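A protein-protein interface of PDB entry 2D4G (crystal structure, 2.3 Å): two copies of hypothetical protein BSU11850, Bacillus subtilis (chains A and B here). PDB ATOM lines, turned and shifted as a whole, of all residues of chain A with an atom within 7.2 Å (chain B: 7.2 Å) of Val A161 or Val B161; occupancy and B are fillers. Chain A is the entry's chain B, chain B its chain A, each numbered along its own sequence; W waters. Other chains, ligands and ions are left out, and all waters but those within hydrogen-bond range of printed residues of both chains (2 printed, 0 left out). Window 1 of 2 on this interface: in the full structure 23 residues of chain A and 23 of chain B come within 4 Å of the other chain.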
ATOM      1  N   VAL A   6       2.687   2.466   8.174  1.00  0.00           N
ATOM      2  CA  VAL A   6       3.271   1.139   8.154  1.00  0.00           C
ATOM      3  C   VAL A   6       4.449   1.017   7.209  1.00  0.00           C
ATOM      4  O   VAL A   6       4.767   1.934   6.450  1.00  0.00           O
ATOM      5  CB  VAL A   6       2.233   0.093   7.694  1.00  0.00           C
ATOM      6  CG1 VAL A   6       0.879   0.364   8.343  1.00  0.00           C
ATOM      7  CG2 VAL A   6       2.108   0.123   6.169  1.00  0.00           C
ATOM      8  N   PHE A   8       5.986  -1.591   4.251  1.00  0.00           N
ATOM      9  CA  PHE A   8       5.608  -2.676   3.370  1.00  0.00           C
ATOM     10  C   PHE A   8       6.929  -3.354   3.042  1.00  0.00           C
ATOM     11  O   PHE A   8       7.845  -2.723   2.508  1.00  0.00           O
ATOM     12  CB  PHE A   8       4.929  -2.145   2.103  1.00  0.00           C
ATOM     13  CG  PHE A   8       3.466  -1.833   2.284  1.00  0.00           C
ATOM     14  CD1 PHE A   8       2.949  -0.595   1.911  1.00  0.00           C
ATOM     15  CD2 PHE A   8       2.600  -2.785   2.824  1.00  0.00           C
ATOM     16  CE1 PHE A   8       1.587  -0.310   2.072  1.00  0.00           C
ATOM     17  CE2 PHE A   8       1.238  -2.510   2.990  1.00  0.00           C
ATOM     18  CZ  PHE A   8       0.731  -1.275   2.614  1.00  0.00           C
ATOM     19  N   GLN A  14       6.053 -10.556   1.485  1.00  0.00           N
ATOM     20  CA  GLN A  14       4.614 -10.335   1.396  1.00  0.00           C
ATOM     21  C   GLN A  14       3.956 -11.624   0.922  1.00  0.00           C
ATOM     22  O   GLN A  14       2.929 -12.040   1.470  1.00  0.00           O
ATOM     23  CB  GLN A  14       4.279  -9.188   0.439  1.00  0.00           C
ATOM     24  CG  GLN A  14       4.509  -7.799   1.021  1.00  0.00           C
ATOM     25  CD  GLN A  14       4.121  -6.703   0.050  1.00  0.00           C
ATOM     26  OE1 GLN A  14       2.935  -6.470  -0.206  1.00  0.00           O
ATOM     27  NE2 GLN A  14       5.118  -6.034  -0.513  1.00  0.00           N
ATOM     28  N   PRO A  32      -2.204  -4.963   2.196  1.00  0.00           N
ATOM     29  CA  PRO A  32      -1.104  -5.901   1.942  1.00  0.00           C
ATOM     30  C   PRO A  32      -0.351  -6.237   3.223  1.00  0.00           C
ATOM     31  O   PRO A  32      -0.471  -5.528   4.218  1.00  0.00           O
ATOM     32  CB  PRO A  32      -0.218  -5.137   0.955  1.00  0.00           C
ATOM     33  CG  PRO A  32      -1.179  -4.202   0.275  1.00  0.00           C
ATOM     34  CD  PRO A  32      -2.021  -3.726   1.418  1.00  0.00           C
ATOM     35  N   ARG A 147      11.582   2.884   3.256  1.00  0.00           N
ATOM     36  CA  ARG A 147      10.479   3.846   3.210  1.00  0.00           C
ATOM     37  C   ARG A 147       9.290   3.367   4.020  1.00  0.00           C
ATOM     38  O   ARG A 147       9.210   2.193   4.374  1.00  0.00           O
ATOM     39  CB  ARG A 147      10.032   4.068   1.756  1.00  0.00           C
ATOM     40  CG  ARG A 147       9.325   2.861   1.120  1.00  0.00           C
ATOM     41  CD  ARG A 147       9.222   3.011  -0.402  1.00  0.00           C
ATOM     42  NE  ARG A 147      10.547   3.026  -1.015  1.00  0.00           N
ATOM     43  CZ  ARG A 147      10.823   3.510  -2.221  1.00  0.00           C
ATOM     44  NH1 ARG A 147       9.861   4.031  -2.976  1.00  0.00           N
ATOM     45  NH2 ARG A 147      12.077   3.494  -2.663  1.00  0.00           N
ATOM     46  N   PHE A 148       8.383   4.284   4.336  1.00  0.00           N
ATOM     47  CA  PHE A 148       7.165   3.920   5.047  1.00  0.00           C
ATOM     48  C   PHE A 148       5.990   4.627   4.378  1.00  0.00           C
ATOM     49  O   PHE A 148       6.177   5.625   3.677  1.00  0.00           O
ATOM     50  CB  PHE A 148       7.256   4.224   6.560  1.00  0.00           C
ATOM     51  CG  PHE A 148       7.445   5.674   6.913  1.00  0.00           C
ATOM     52  CD1 PHE A 148       6.445   6.614   6.677  1.00  0.00           C
ATOM     53  CD2 PHE A 148       8.602   6.084   7.574  1.00  0.00           C
ATOM     54  CE1 PHE A 148       6.591   7.941   7.102  1.00  0.00           C
ATOM     55  CE2 PHE A 148       8.759   7.407   8.004  1.00  0.00           C
ATOM     56  CZ  PHE A 148       7.750   8.335   7.768  1.00  0.00           C
ATOM     57  N   HIS A 149       4.787   4.095   4.566  1.00  0.00           N
ATOM     58  CA  HIS A 149       3.611   4.665   3.928  1.00  0.00           C
ATOM     59  C   HIS A 149       2.545   5.179   4.869  1.00  0.00           C
ATOM     60  O   HIS A 149       2.303   4.603   5.929  1.00  0.00           O
ATOM     61  CB  HIS A 149       2.953   3.633   3.018  1.00  0.00           C
ATOM     62  CG  HIS A 149       3.893   2.981   2.057  1.00  0.00           C
ATOM     63  ND1 HIS A 149       4.877   2.105   2.459  1.00  0.00           N
ATOM     64  CD2 HIS A 149       3.979   3.050   0.708  1.00  0.00           C
ATOM     65  CE1 HIS A 149       5.527   1.659   1.398  1.00  0.00           C
ATOM     66  NE2 HIS A 149       5.002   2.219   0.323  1.00  0.00           N
ATOM     67  N   LEU A 150       1.903   6.265   4.454  1.00  0.00           N
ATOM     68  CA  LEU A 150       0.811   6.858   5.204  1.00  0.00           C
ATOM     69  C   LEU A 150      -0.431   6.371   4.465  1.00  0.00           C
ATOM     70  O   LEU A 150      -0.519   6.493   3.238  1.00  0.00           O
ATOM     71  CB  LEU A 150       0.878   8.392   5.154  1.00  0.00           C
ATOM     72  CG  LEU A 150      -0.303   9.112   5.818  1.00  0.00           C
ATOM     73  CD1 LEU A 150      -0.230   8.937   7.326  1.00  0.00           C
ATOM     74  CD2 LEU A 150      -0.280  10.589   5.458  1.00  0.00           C
ATOM     75  N   LEU A 151      -1.381   5.816   5.204  1.00  0.00           N
ATOM     76  CA  LEU A 151      -2.597   5.301   4.600  1.00  0.00           C
ATOM     77  C   LEU A 151      -3.838   5.838   5.297  1.00  0.00           C
ATOM     78  O   LEU A 151      -3.757   6.415   6.380  1.00  0.00           O
ATOM     79  CB  LEU A 151      -2.600   3.778   4.695  1.00  0.00           C
ATOM     80  CG  LEU A 151      -1.295   3.073   4.320  1.00  0.00           C
ATOM     81  CD1 LEU A 151      -0.949   2.048   5.387  1.00  0.00           C
ATOM     82  CD2 LEU A 151      -1.435   2.415   2.971  1.00  0.00           C
ATOM     83  N   TYR A 152      -4.989   5.650   4.661  1.00  0.00           N
ATOM     84  CA  TYR A 152      -6.257   6.060   5.237  1.00  0.00           C
ATOM     85  C   TYR A 152      -7.255   4.940   4.960  1.00  0.00           C
ATOM     86  O   TYR A 152      -7.145   4.228   3.953  1.00  0.00           O
ATOM     87  CB  TYR A 152      -6.718   7.406   4.661  1.00  0.00           C
ATOM     88  CG  TYR A 152      -6.923   7.459   3.168  1.00  0.00           C
ATOM     89  CD1 TYR A 152      -8.116   7.024   2.592  1.00  0.00           C
ATOM     90  CD2 TYR A 152      -5.934   7.971   2.329  1.00  0.00           C
ATOM     91  CE1 TYR A 152      -8.320   7.100   1.222  1.00  0.00           C
ATOM     92  CE2 TYR A 152      -6.129   8.051   0.957  1.00  0.00           C
ATOM     93  CZ  TYR A 152      -7.324   7.614   0.413  1.00  0.00           C
ATOM     94  OH  TYR A 152      -7.525   7.693  -0.941  1.00  0.00           O
ATOM     95  N   TRP A 159      -7.543  -0.364   3.197  1.00  0.00           N
ATOM     96  CA  TRP A 159      -6.630   0.762   3.325  1.00  0.00           C
ATOM     97  C   TRP A 159      -5.978   1.196   2.015  1.00  0.00           C
ATOM     98  O   TRP A 159      -5.471   0.368   1.257  1.00  0.00           O
ATOM     99  CB  TRP A 159      -5.536   0.433   4.348  1.00  0.00           C
ATOM    100  CG  TRP A 159      -6.058   0.151   5.730  1.00  0.00           C
ATOM    101  CD1 TRP A 159      -6.622  -1.008   6.175  1.00  0.00           C
ATOM    102  CD2 TRP A 159      -6.057   1.046   6.849  1.00  0.00           C
ATOM    103  NE1 TRP A 159      -6.989  -0.887   7.488  1.00  0.00           N
ATOM    104  CE2 TRP A 159      -6.677   0.360   7.912  1.00  0.00           C
ATOM    105  CE3 TRP A 159      -5.663   2.368   7.022  1.00  0.00           C
ATOM    106  CZ2 TRP A 159      -6.827   0.947   9.157  1.00  0.00           C
ATOM    107  CZ3 TRP A 159      -5.836   2.942   8.260  1.00  0.00           C
ATOM    108  CH2 TRP A 159      -6.436   2.242   9.302  1.00  0.00           C
ATOM    109  N   THR A 160      -5.979   2.505   1.773  1.00  0.00           N
ATOM    110  CA  THR A 160      -5.400   3.087   0.568  1.00  0.00           C
ATOM    111  C   THR A 160      -4.198   3.959   0.922  1.00  0.00           C
ATOM    112  O   THR A 160      -4.230   4.701   1.900  1.00  0.00           O
ATOM    113  CB  THR A 160      -6.437   3.955  -0.184  1.00  0.00           C
ATOM    114  OG1 THR A 160      -7.563   3.146  -0.549  1.00  0.00           O
ATOM    115  CG2 THR A 160      -5.827   4.551  -1.450  1.00  0.00           C
ATOM    116  N   VAL A 161      -3.136   3.862   0.131  1.00  0.00           N
ATOM    117  CA  VAL A 161      -1.935   4.650   0.381  1.00  0.00           C
ATOM    118  C   VAL A 161      -2.161   6.097  -0.036  1.00  0.00           C
ATOM    119  O   VAL A 161      -2.709   6.357  -1.107  1.00  0.00           O
ATOM    120  CB  VAL A 161      -0.719   4.108  -0.418  1.00  0.00           C
ATOM    121  CG1 VAL A 161       0.512   4.978  -0.166  1.00  0.00           C
ATOM    122  CG2 VAL A 161      -0.439   2.673  -0.033  1.00  0.00           C
ATOM    123  N   TYR A 162      -1.742   7.034   0.810  1.00  0.00           N
ATOM    124  CA  TYR A 162      -1.878   8.453   0.494  1.00  0.00           C
ATOM    125  C   TYR A 162      -0.515   8.967   0.028  1.00  0.00           C
ATOM    126  O   TYR A 162      -0.404   9.593  -1.029  1.00  0.00           O
ATOM    127  CB  TYR A 162      -2.347   9.237   1.726  1.00  0.00           C
ATOM    128  CG  TYR A 162      -2.535  10.722   1.485  1.00  0.00           C
ATOM    129  CD1 TYR A 162      -3.431  11.191   0.517  1.00  0.00           C
ATOM    130  CD2 TYR A 162      -1.810  11.664   2.220  1.00  0.00           C
ATOM    131  CE1 TYR A 162      -3.596  12.565   0.288  1.00  0.00           C
ATOM    132  CE2 TYR A 162      -1.966  13.033   2.000  1.00  0.00           C
ATOM    133  CZ  TYR A 162      -2.857  13.478   1.034  1.00  0.00           C
ATOM    134  OH  TYR A 162      -2.983  14.835   0.819  1.00  0.00           O
ATOM    135  N   GLU A 163       0.524   8.681   0.810  1.00  0.00           N
ATOM    136  CA  GLU A 163       1.866   9.123   0.466  1.00  0.00           C
ATOM    137  C   GLU A 163       2.968   8.173   0.954  1.00  0.00           C
ATOM    138  O   GLU A 163       2.817   7.477   1.965  1.00  0.00           O
ATOM    139  CB  GLU A 163       2.102  10.529   1.029  1.00  0.00           C
ATOM    140  CG  GLU A 163       3.067  11.369   0.208  1.00  0.00           C
ATOM    141  CD  GLU A 163       3.180  12.802   0.710  1.00  0.00           C
ATOM    142  OE1 GLU A 163       2.131  13.461   0.893  1.00  0.00           O
ATOM    143  OE2 GLU A 163       4.321  13.273   0.911  1.00  0.00           O
ATOM    144  N   THR A 164       4.071   8.141   0.213  1.00  0.00           N
ATOM    145  CA  THR A 164       5.213   7.305   0.555  1.00  0.00           C
ATOM    146  C   THR A 164       6.299   8.232   1.070  1.00  0.00           C
ATOM    147  O   THR A 164       6.393   9.376   0.634  1.00  0.00           O
ATOM    148  CB  THR A 164       5.751   6.533  -0.678  1.00  0.00           C
ATOM    149  OG1 THR A 164       6.035   7.455  -1.737  1.00  0.00           O
ATOM    150  CG2 THR A 164       4.725   5.534  -1.169  1.00  0.00           C
ATOM    151  N   VAL B   6      -0.953   4.468 -11.249  1.00  0.00           N
ATOM    152  CA  VAL B   6      -2.427   4.801 -11.308  1.00  0.00           C
ATOM    153  C   VAL B   6      -2.745   5.999 -10.448  1.00  0.00           C
ATOM    154  O   VAL B   6      -1.859   6.497  -9.798  1.00  0.00           O
ATOM    155  CB  VAL B   6      -3.455   3.693 -10.669  1.00  0.00           C
ATOM    156  CG1 VAL B   6      -3.504   2.322 -11.365  1.00  0.00           C
ATOM    157  CG2 VAL B   6      -3.170   3.448  -9.189  1.00  0.00           C
ATOM    158  N   PHE B   8      -5.392   7.320  -7.296  1.00  0.00           N
ATOM    159  CA  PHE B   8      -6.313   6.854  -6.277  1.00  0.00           C
ATOM    160  C   PHE B   8      -7.091   8.118  -5.957  1.00  0.00           C
ATOM    161  O   PHE B   8      -6.524   9.091  -5.458  1.00  0.00           O
ATOM    162  CB  PHE B   8      -5.559   6.368  -5.035  1.00  0.00           C
ATOM    163  CG  PHE B   8      -4.922   5.008  -5.197  1.00  0.00           C
ATOM    164  CD1 PHE B   8      -3.596   4.801  -4.829  1.00  0.00           C
ATOM    165  CD2 PHE B   8      -5.657   3.928  -5.668  1.00  0.00           C
ATOM    166  CE1 PHE B   8      -3.015   3.540  -4.926  1.00  0.00           C
ATOM    167  CE2 PHE B   8      -5.080   2.662  -5.766  1.00  0.00           C
ATOM    168  CZ  PHE B   8      -3.759   2.472  -5.392  1.00  0.00           C
ATOM    169  N   GLN B  14     -13.908   6.264  -4.015  1.00  0.00           N
ATOM    170  CA  GLN B  14     -13.525   4.866  -3.871  1.00  0.00           C
ATOM    171  C   GLN B  14     -14.674   4.077  -3.234  1.00  0.00           C
ATOM    172  O   GLN B  14     -15.033   2.988  -3.697  1.00  0.00           O
ATOM    173  CB  GLN B  14     -12.272   4.741  -2.998  1.00  0.00           C
ATOM    174  CG  GLN B  14     -11.024   5.367  -3.581  1.00  0.00           C
ATOM    175  CD  GLN B  14      -9.816   5.180  -2.678  1.00  0.00           C
ATOM    176  OE1 GLN B  14      -9.468   4.056  -2.315  1.00  0.00           O
ATOM    177  NE2 GLN B  14      -9.173   6.279  -2.307  1.00  0.00           N
ATOM    178  N   PRO B  32      -7.552  -1.072  -4.432  1.00  0.00           N
ATOM    179  CA  PRO B  32      -8.675  -0.142  -4.254  1.00  0.00           C
ATOM    180  C   PRO B  32      -9.048   0.595  -5.546  1.00  0.00           C
ATOM    181  O   PRO B  32      -8.259   0.640  -6.489  1.00  0.00           O
ATOM    182  CB  PRO B  32      -8.175   0.798  -3.157  1.00  0.00           C
ATOM    183  CG  PRO B  32      -6.687   0.807  -3.366  1.00  0.00           C
ATOM    184  CD  PRO B  32      -6.380  -0.648  -3.646  1.00  0.00           C
ATOM    185  N   ARG B 147      -1.748  13.512  -7.268  1.00  0.00           N
ATOM    186  CA  ARG B 147      -0.672  12.527  -7.175  1.00  0.00           C
ATOM    187  C   ARG B 147      -1.008  11.189  -7.830  1.00  0.00           C
ATOM    188  O   ARG B 147      -2.174  10.822  -7.947  1.00  0.00           O
ATOM    189  CB  ARG B 147      -0.341  12.275  -5.697  1.00  0.00           C
ATOM    190  CG  ARG B 147      -1.457  11.550  -4.923  1.00  0.00           C
ATOM    191  CD  ARG B 147      -1.166  11.493  -3.426  1.00  0.00           C
ATOM    192  NE  ARG B 147      -1.194  12.823  -2.823  1.00  0.00           N
ATOM    193  CZ  ARG B 147      -0.529  13.163  -1.724  1.00  0.00           C
ATOM    194  NH1 ARG B 147       0.223  12.272  -1.096  1.00  0.00           N
ATOM    195  NH2 ARG B 147      -0.612  14.401  -1.253  1.00  0.00           N
ATOM    196  N   PHE B 148       0.022  10.462  -8.255  1.00  0.00           N
ATOM    197  CA  PHE B 148      -0.188   9.146  -8.840  1.00  0.00           C
ATOM    198  C   PHE B 148       0.757   8.168  -8.157  1.00  0.00           C
ATOM    199  O   PHE B 148       1.751   8.575  -7.553  1.00  0.00           O
ATOM    200  CB  PHE B 148      -0.011   9.164 -10.371  1.00  0.00           C
ATOM    201  CG  PHE B 148       1.355   9.593 -10.854  1.00  0.00           C
ATOM    202  CD1 PHE B 148       2.411   8.682 -10.928  1.00  0.00           C
ATOM    203  CD2 PHE B 148       1.561  10.894 -11.319  1.00  0.00           C
ATOM    204  CE1 PHE B 148       3.648   9.059 -11.465  1.00  0.00           C
ATOM    205  CE2 PHE B 148       2.792  11.278 -11.856  1.00  0.00           C
ATOM    206  CZ  PHE B 148       3.835  10.359 -11.931  1.00  0.00           C
ATOM    207  N   HIS B 149       0.434   6.884  -8.225  1.00  0.00           N
ATOM    208  CA  HIS B 149       1.245   5.876  -7.562  1.00  0.00           C
ATOM    209  C   HIS B 149       1.806   4.826  -8.498  1.00  0.00           C
ATOM    210  O   HIS B 149       1.230   4.534  -9.545  1.00  0.00           O
ATOM    211  CB  HIS B 149       0.418   5.172  -6.483  1.00  0.00           C
ATOM    212  CG  HIS B 149      -0.230   6.105  -5.514  1.00  0.00           C
ATOM    213  ND1 HIS B 149      -1.253   6.957  -5.869  1.00  0.00           N
ATOM    214  CD2 HIS B 149       0.022   6.346  -4.206  1.00  0.00           C
ATOM    215  CE1 HIS B 149      -1.601   7.685  -4.823  1.00  0.00           C
ATOM    216  NE2 HIS B 149      -0.841   7.333  -3.801  1.00  0.00           N
ATOM    217  N   LEU B 150       2.946   4.270  -8.109  1.00  0.00           N
ATOM    218  CA  LEU B 150       3.584   3.214  -8.879  1.00  0.00           C
ATOM    219  C   LEU B 150       3.419   1.998  -7.997  1.00  0.00           C
ATOM    220  O   LEU B 150       3.674   2.066  -6.802  1.00  0.00           O
ATOM    221  CB  LEU B 150       5.074   3.493  -9.081  1.00  0.00           C
ATOM    222  CG  LEU B 150       5.912   2.324  -9.615  1.00  0.00           C
ATOM    223  CD1 LEU B 150       5.398   1.887 -10.981  1.00  0.00           C
ATOM    224  CD2 LEU B 150       7.386   2.756  -9.694  1.00  0.00           C
ATOM    225  N   LEU B 151       2.990   0.881  -8.554  1.00  0.00           N
ATOM    226  CA  LEU B 151       2.818  -0.274  -7.698  1.00  0.00           C
ATOM    227  C   LEU B 151       3.317  -1.529  -8.445  1.00  0.00           C
ATOM    228  O   LEU B 151       3.568  -1.491  -9.660  1.00  0.00           O
ATOM    229  CB  LEU B 151       1.320  -0.395  -7.302  1.00  0.00           C
ATOM    230  CG  LEU B 151       0.389   0.638  -6.566  1.00  0.00           C
ATOM    231  CD1 LEU B 151      -0.091   1.693  -7.524  1.00  0.00           C
ATOM    232  CD2 LEU B 151      -0.856  -0.016  -6.246  1.00  0.00           C
ATOM    233  N   TYR B 152       3.494  -2.623  -7.708  1.00  0.00           N
ATOM    234  CA  TYR B 152       3.950  -3.888  -8.287  1.00  0.00           C
ATOM    235  C   TYR B 152       3.028  -5.015  -7.822  1.00  0.00           C
ATOM    236  O   TYR B 152       2.429  -4.939  -6.745  1.00  0.00           O
ATOM    237  CB  TYR B 152       5.397  -4.173  -7.879  1.00  0.00           C
ATOM    238  CG  TYR B 152       5.632  -4.149  -6.388  1.00  0.00           C
ATOM    239  CD1 TYR B 152       5.495  -5.303  -5.619  1.00  0.00           C
ATOM    240  CD2 TYR B 152       5.970  -2.960  -5.739  1.00  0.00           C
ATOM    241  CE1 TYR B 152       5.688  -5.276  -4.237  1.00  0.00           C
ATOM    242  CE2 TYR B 152       6.163  -2.919  -4.354  1.00  0.00           C
ATOM    243  CZ  TYR B 152       6.023  -4.078  -3.611  1.00  0.00           C
ATOM    244  OH  TYR B 152       6.215  -4.036  -2.246  1.00  0.00           O
ATOM    245  N   TRP B 159      -2.001  -5.759  -5.765  1.00  0.00           N
ATOM    246  CA  TRP B 159      -0.987  -4.750  -6.042  1.00  0.00           C
ATOM    247  C   TRP B 159      -0.621  -3.935  -4.796  1.00  0.00           C
ATOM    248  O   TRP B 159      -1.498  -3.527  -4.036  1.00  0.00           O
ATOM    249  CB  TRP B 159      -1.476  -3.796  -7.143  1.00  0.00           C
ATOM    250  CG  TRP B 159      -1.765  -4.468  -8.468  1.00  0.00           C
ATOM    251  CD1 TRP B 159      -2.876  -5.198  -8.796  1.00  0.00           C
ATOM    252  CD2 TRP B 159      -0.936  -4.442  -9.642  1.00  0.00           C
ATOM    253  NE1 TRP B 159      -2.783  -5.659 -10.093  1.00  0.00           N
ATOM    254  CE2 TRP B 159      -1.610  -5.251 -10.611  1.00  0.00           C
ATOM    255  CE3 TRP B 159       0.324  -3.923  -9.922  1.00  0.00           C
ATOM    256  CZ2 TRP B 159      -1.072  -5.414 -11.898  1.00  0.00           C
ATOM    257  CZ3 TRP B 159       0.844  -4.107 -11.195  1.00  0.00           C
ATOM    258  CH2 TRP B 159       0.166  -4.887 -12.150  1.00  0.00           C
ATOM    259  N   THR B 160       0.678  -3.704  -4.602  1.00  0.00           N
ATOM    260  CA  THR B 160       1.187  -2.931  -3.470  1.00  0.00           C
ATOM    261  C   THR B 160       1.852  -1.652  -3.986  1.00  0.00           C
ATOM    262  O   THR B 160       2.494  -1.666  -5.032  1.00  0.00           O
ATOM    263  CB  THR B 160       2.250  -3.720  -2.669  1.00  0.00           C
ATOM    264  OG1 THR B 160       1.678  -4.934  -2.160  1.00  0.00           O
ATOM    265  CG2 THR B 160       2.779  -2.875  -1.511  1.00  0.00           C
ATOM    266  N   VAL B 161       1.699  -0.556  -3.248  1.00  0.00           N
ATOM    267  CA  VAL B 161       2.284   0.728  -3.628  1.00  0.00           C
ATOM    268  C   VAL B 161       3.780   0.784  -3.342  1.00  0.00           C
ATOM    269  O   VAL B 161       4.217   0.530  -2.220  1.00  0.00           O
ATOM    270  CB  VAL B 161       1.608   1.900  -2.867  1.00  0.00           C
ATOM    271  CG1 VAL B 161       2.379   3.203  -3.105  1.00  0.00           C
ATOM    272  CG2 VAL B 161       0.166   2.048  -3.316  1.00  0.00           C
ATOM    273  N   TYR B 162       4.566   1.121  -4.358  1.00  0.00           N
ATOM    274  CA  TYR B 162       6.006   1.221  -4.174  1.00  0.00           C
ATOM    275  C   TYR B 162       6.360   2.668  -3.869  1.00  0.00           C
ATOM    276  O   TYR B 162       7.081   2.947  -2.910  1.00  0.00           O
ATOM    277  CB  TYR B 162       6.747   0.752  -5.430  1.00  0.00           C
ATOM    278  CG  TYR B 162       8.259   0.857  -5.332  1.00  0.00           C
ATOM    279  CD1 TYR B 162       8.960   0.240  -4.294  1.00  0.00           C
ATOM    280  CD2 TYR B 162       8.988   1.555  -6.292  1.00  0.00           C
ATOM    281  CE1 TYR B 162      10.357   0.317  -4.219  1.00  0.00           C
ATOM    282  CE2 TYR B 162      10.379   1.635  -6.229  1.00  0.00           C
ATOM    283  CZ  TYR B 162      11.056   1.015  -5.196  1.00  0.00           C
ATOM    284  OH  TYR B 162      12.427   1.085  -5.157  1.00  0.00           O
ATOM    285  N   GLU B 163       5.834   3.591  -4.671  1.00  0.00           N
ATOM    286  CA  GLU B 163       6.123   5.004  -4.463  1.00  0.00           C
ATOM    287  C   GLU B 163       5.008   5.923  -4.959  1.00  0.00           C
ATOM    288  O   GLU B 163       4.303   5.601  -5.914  1.00  0.00           O
ATOM    289  CB  GLU B 163       7.442   5.363  -5.161  1.00  0.00           C
ATOM    290  CG  GLU B 163       8.119   6.621  -4.641  1.00  0.00           C
ATOM    291  CD  GLU B 163       9.524   6.796  -5.203  1.00  0.00           C
ATOM    292  OE1 GLU B 163      10.339   5.855  -5.102  1.00  0.00           O
ATOM    293  OE2 GLU B 163       9.819   7.878  -5.745  1.00  0.00           O
ATOM    294  N   THR B 164       4.872   7.075  -4.303  1.00  0.00           N
ATOM    295  CA  THR B 164       3.863   8.072  -4.650  1.00  0.00           C
ATOM    296  C   THR B 164       4.535   9.335  -5.170  1.00  0.00           C
ATOM    297  O   THR B 164       5.526   9.793  -4.604  1.00  0.00           O
ATOM    298  CB  THR B 164       3.018   8.460  -3.426  1.00  0.00           C
ATOM    299  OG1 THR B 164       2.287   7.318  -2.973  1.00  0.00           O
ATOM    300  CG2 THR B 164       2.053   9.590  -3.774  1.00  0.00           C
HETATM  301  O   HOH W   1       0.827  15.918   0.732  1.00  0.00           O
HETATM  302  O   HOH W   2      12.756   5.172  -4.893  1.00  0.00           O
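Of the 16 printed residues of chain A, 11 touch a printed residue of chain B. Of the 16 printed residues of chain B, 11 touch a printed residue of chain A.
Gln A14 touches Thr B160, and with the chains exchanged Thr A160 touches Gln B14. Pro A32 touches Thr B160, and with the chains exchanged Thr A160 touches Pro B32. Arg A147 touches Tyr B162, and with the chains exchanged Tyr A162 touches Arg B147. Arg A147 touches Glu B163, and with the chains exchanged Glu A163 touches Arg B147. Of the 23 pairs that touch across the chains among the printed residues, 22 have their exchanged pair printed and touching as well.
OG1 of Thr B164 lies close to NE2 of His B149, at 3.2 Å. O of Leu B150 sits at hydrogen-bond distance from N of Tyr B162 (2.8 Å). N of Leu B150 is in hydrogen-bond range of O of Glu B163, at 2.9 Å. The backbone carbonyl oxygen (O) of Leu A150 sits at hydrogen-bond distance from the backbone NH (N) of Tyr A162 (2.8 Å). The backbone carbonyl oxygen (O) of Tyr A152 lies within hydrogen-bond range of the backbone NH (N) of Thr A160 (3.0 Å).
Water W2 lies within hydrogen-bond range of the side-chain carboxylate (OE1) of Glu B163 and the guanidinium group (NH2) of Arg A147. Water W1 lies within hydrogen-bond range of the side-chain carboxylate (OE1) of Glu A163 and the guanidinium group (NH2) of Arg B147.
NE2 of Gln B14 lies within hydrogen-bond range of OH of Tyr A152 (2.6 Å). OE1 of Gln B14 lies within hydrogen-bond range of OG1 of Thr A160 (2.8 Å). The guanidinium group (NH1) of Arg B147 sits at hydrogen-bond distance from the backbone carbonyl oxygen (O) of Tyr A162 (2.8 Å). The guanidinium group (NH1) of Arg B147 is in salt-bridge range of the side-chain carboxylate (OE1) of Glu A163 (3.0 Å). NE2 of His B149 is in hydrogen-bond range of O of Val A161 (3.4 Å). The side-chain hydroxyl of Tyr B152 is in hydrogen-bond range of the side-chain amide nitrogen of Gln A14 (2.9 Å). OG1 of Thr B160 lies within hydrogen-bond range of OE1 of Gln A14, at 2.8 Å. O of Val B161 lies within hydrogen-bond range of NE2 of His A149 (3.2 Å). The backbone carbonyl oxygen (O) of Tyr B162 sits at hydrogen-bond distance from the guanidinium group (NH1) of Arg A147, at 3.0 Å. The guanidinium group (NH1) of Arg A147 is in salt-bridge range of the side-chain carboxylate (OE1) of Glu B163, 2.8 Å away. The backbone NH (N) of Thr B164 lies within hydrogen-bond range of the side-chain hydroxyl (OG1) of Thr A164 (2.8 Å).
Printed residues of chain B within 4 Å of Gln A14: Tyr B152 (2.9 Å) and Thr B160 (2.8 Å). Phe A148 touches none of the printed residues of chain B. Val A161 touches two residues of chain B. Of the printed residues of chain A, Arg B147 touches Tyr A162 (2.8 Å) and Glu A163 (3.0 Å). Of the printed residues of chain A, His B149 touches Val A161 and Tyr A162. Val B161 touches just these residues of chain A: His A149 (3.2 Å), Val A161 (3.4 Å) and Thr A164 (3.8 Å). Printed residues of chain A within 4 Å of Glu B163: Arg A147 (2.8 Å) and Thr A164 (3.6 Å). Of the printed residues of chain A, Thr B164 touches Tyr A162 (3.7 Å), Glu A163 (3.9 Å) and Thr A164 (2.8 Å).
Thr B160 touches Phe A8 (CG2 to CG, 3.99 Å). Pro A32 touches Thr B160 (CB to OG1, 3.7 Å). Tyr B162 touches His A149. Thr A160 touches Phe B8 (CG2 to CG, 3.9 Å). Val A161 touches Val B161. NE2 of His B149 touches O of Tyr A162, 3.6 Å away. Tyr A162 touches Thr B164 (O to CG2, 3.7 Å). Glu A163 touches Thr B164. Thr A164 touches Val B161. Thr A164 touches Glu B163 (CG2 to CA, 3.6 Å).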
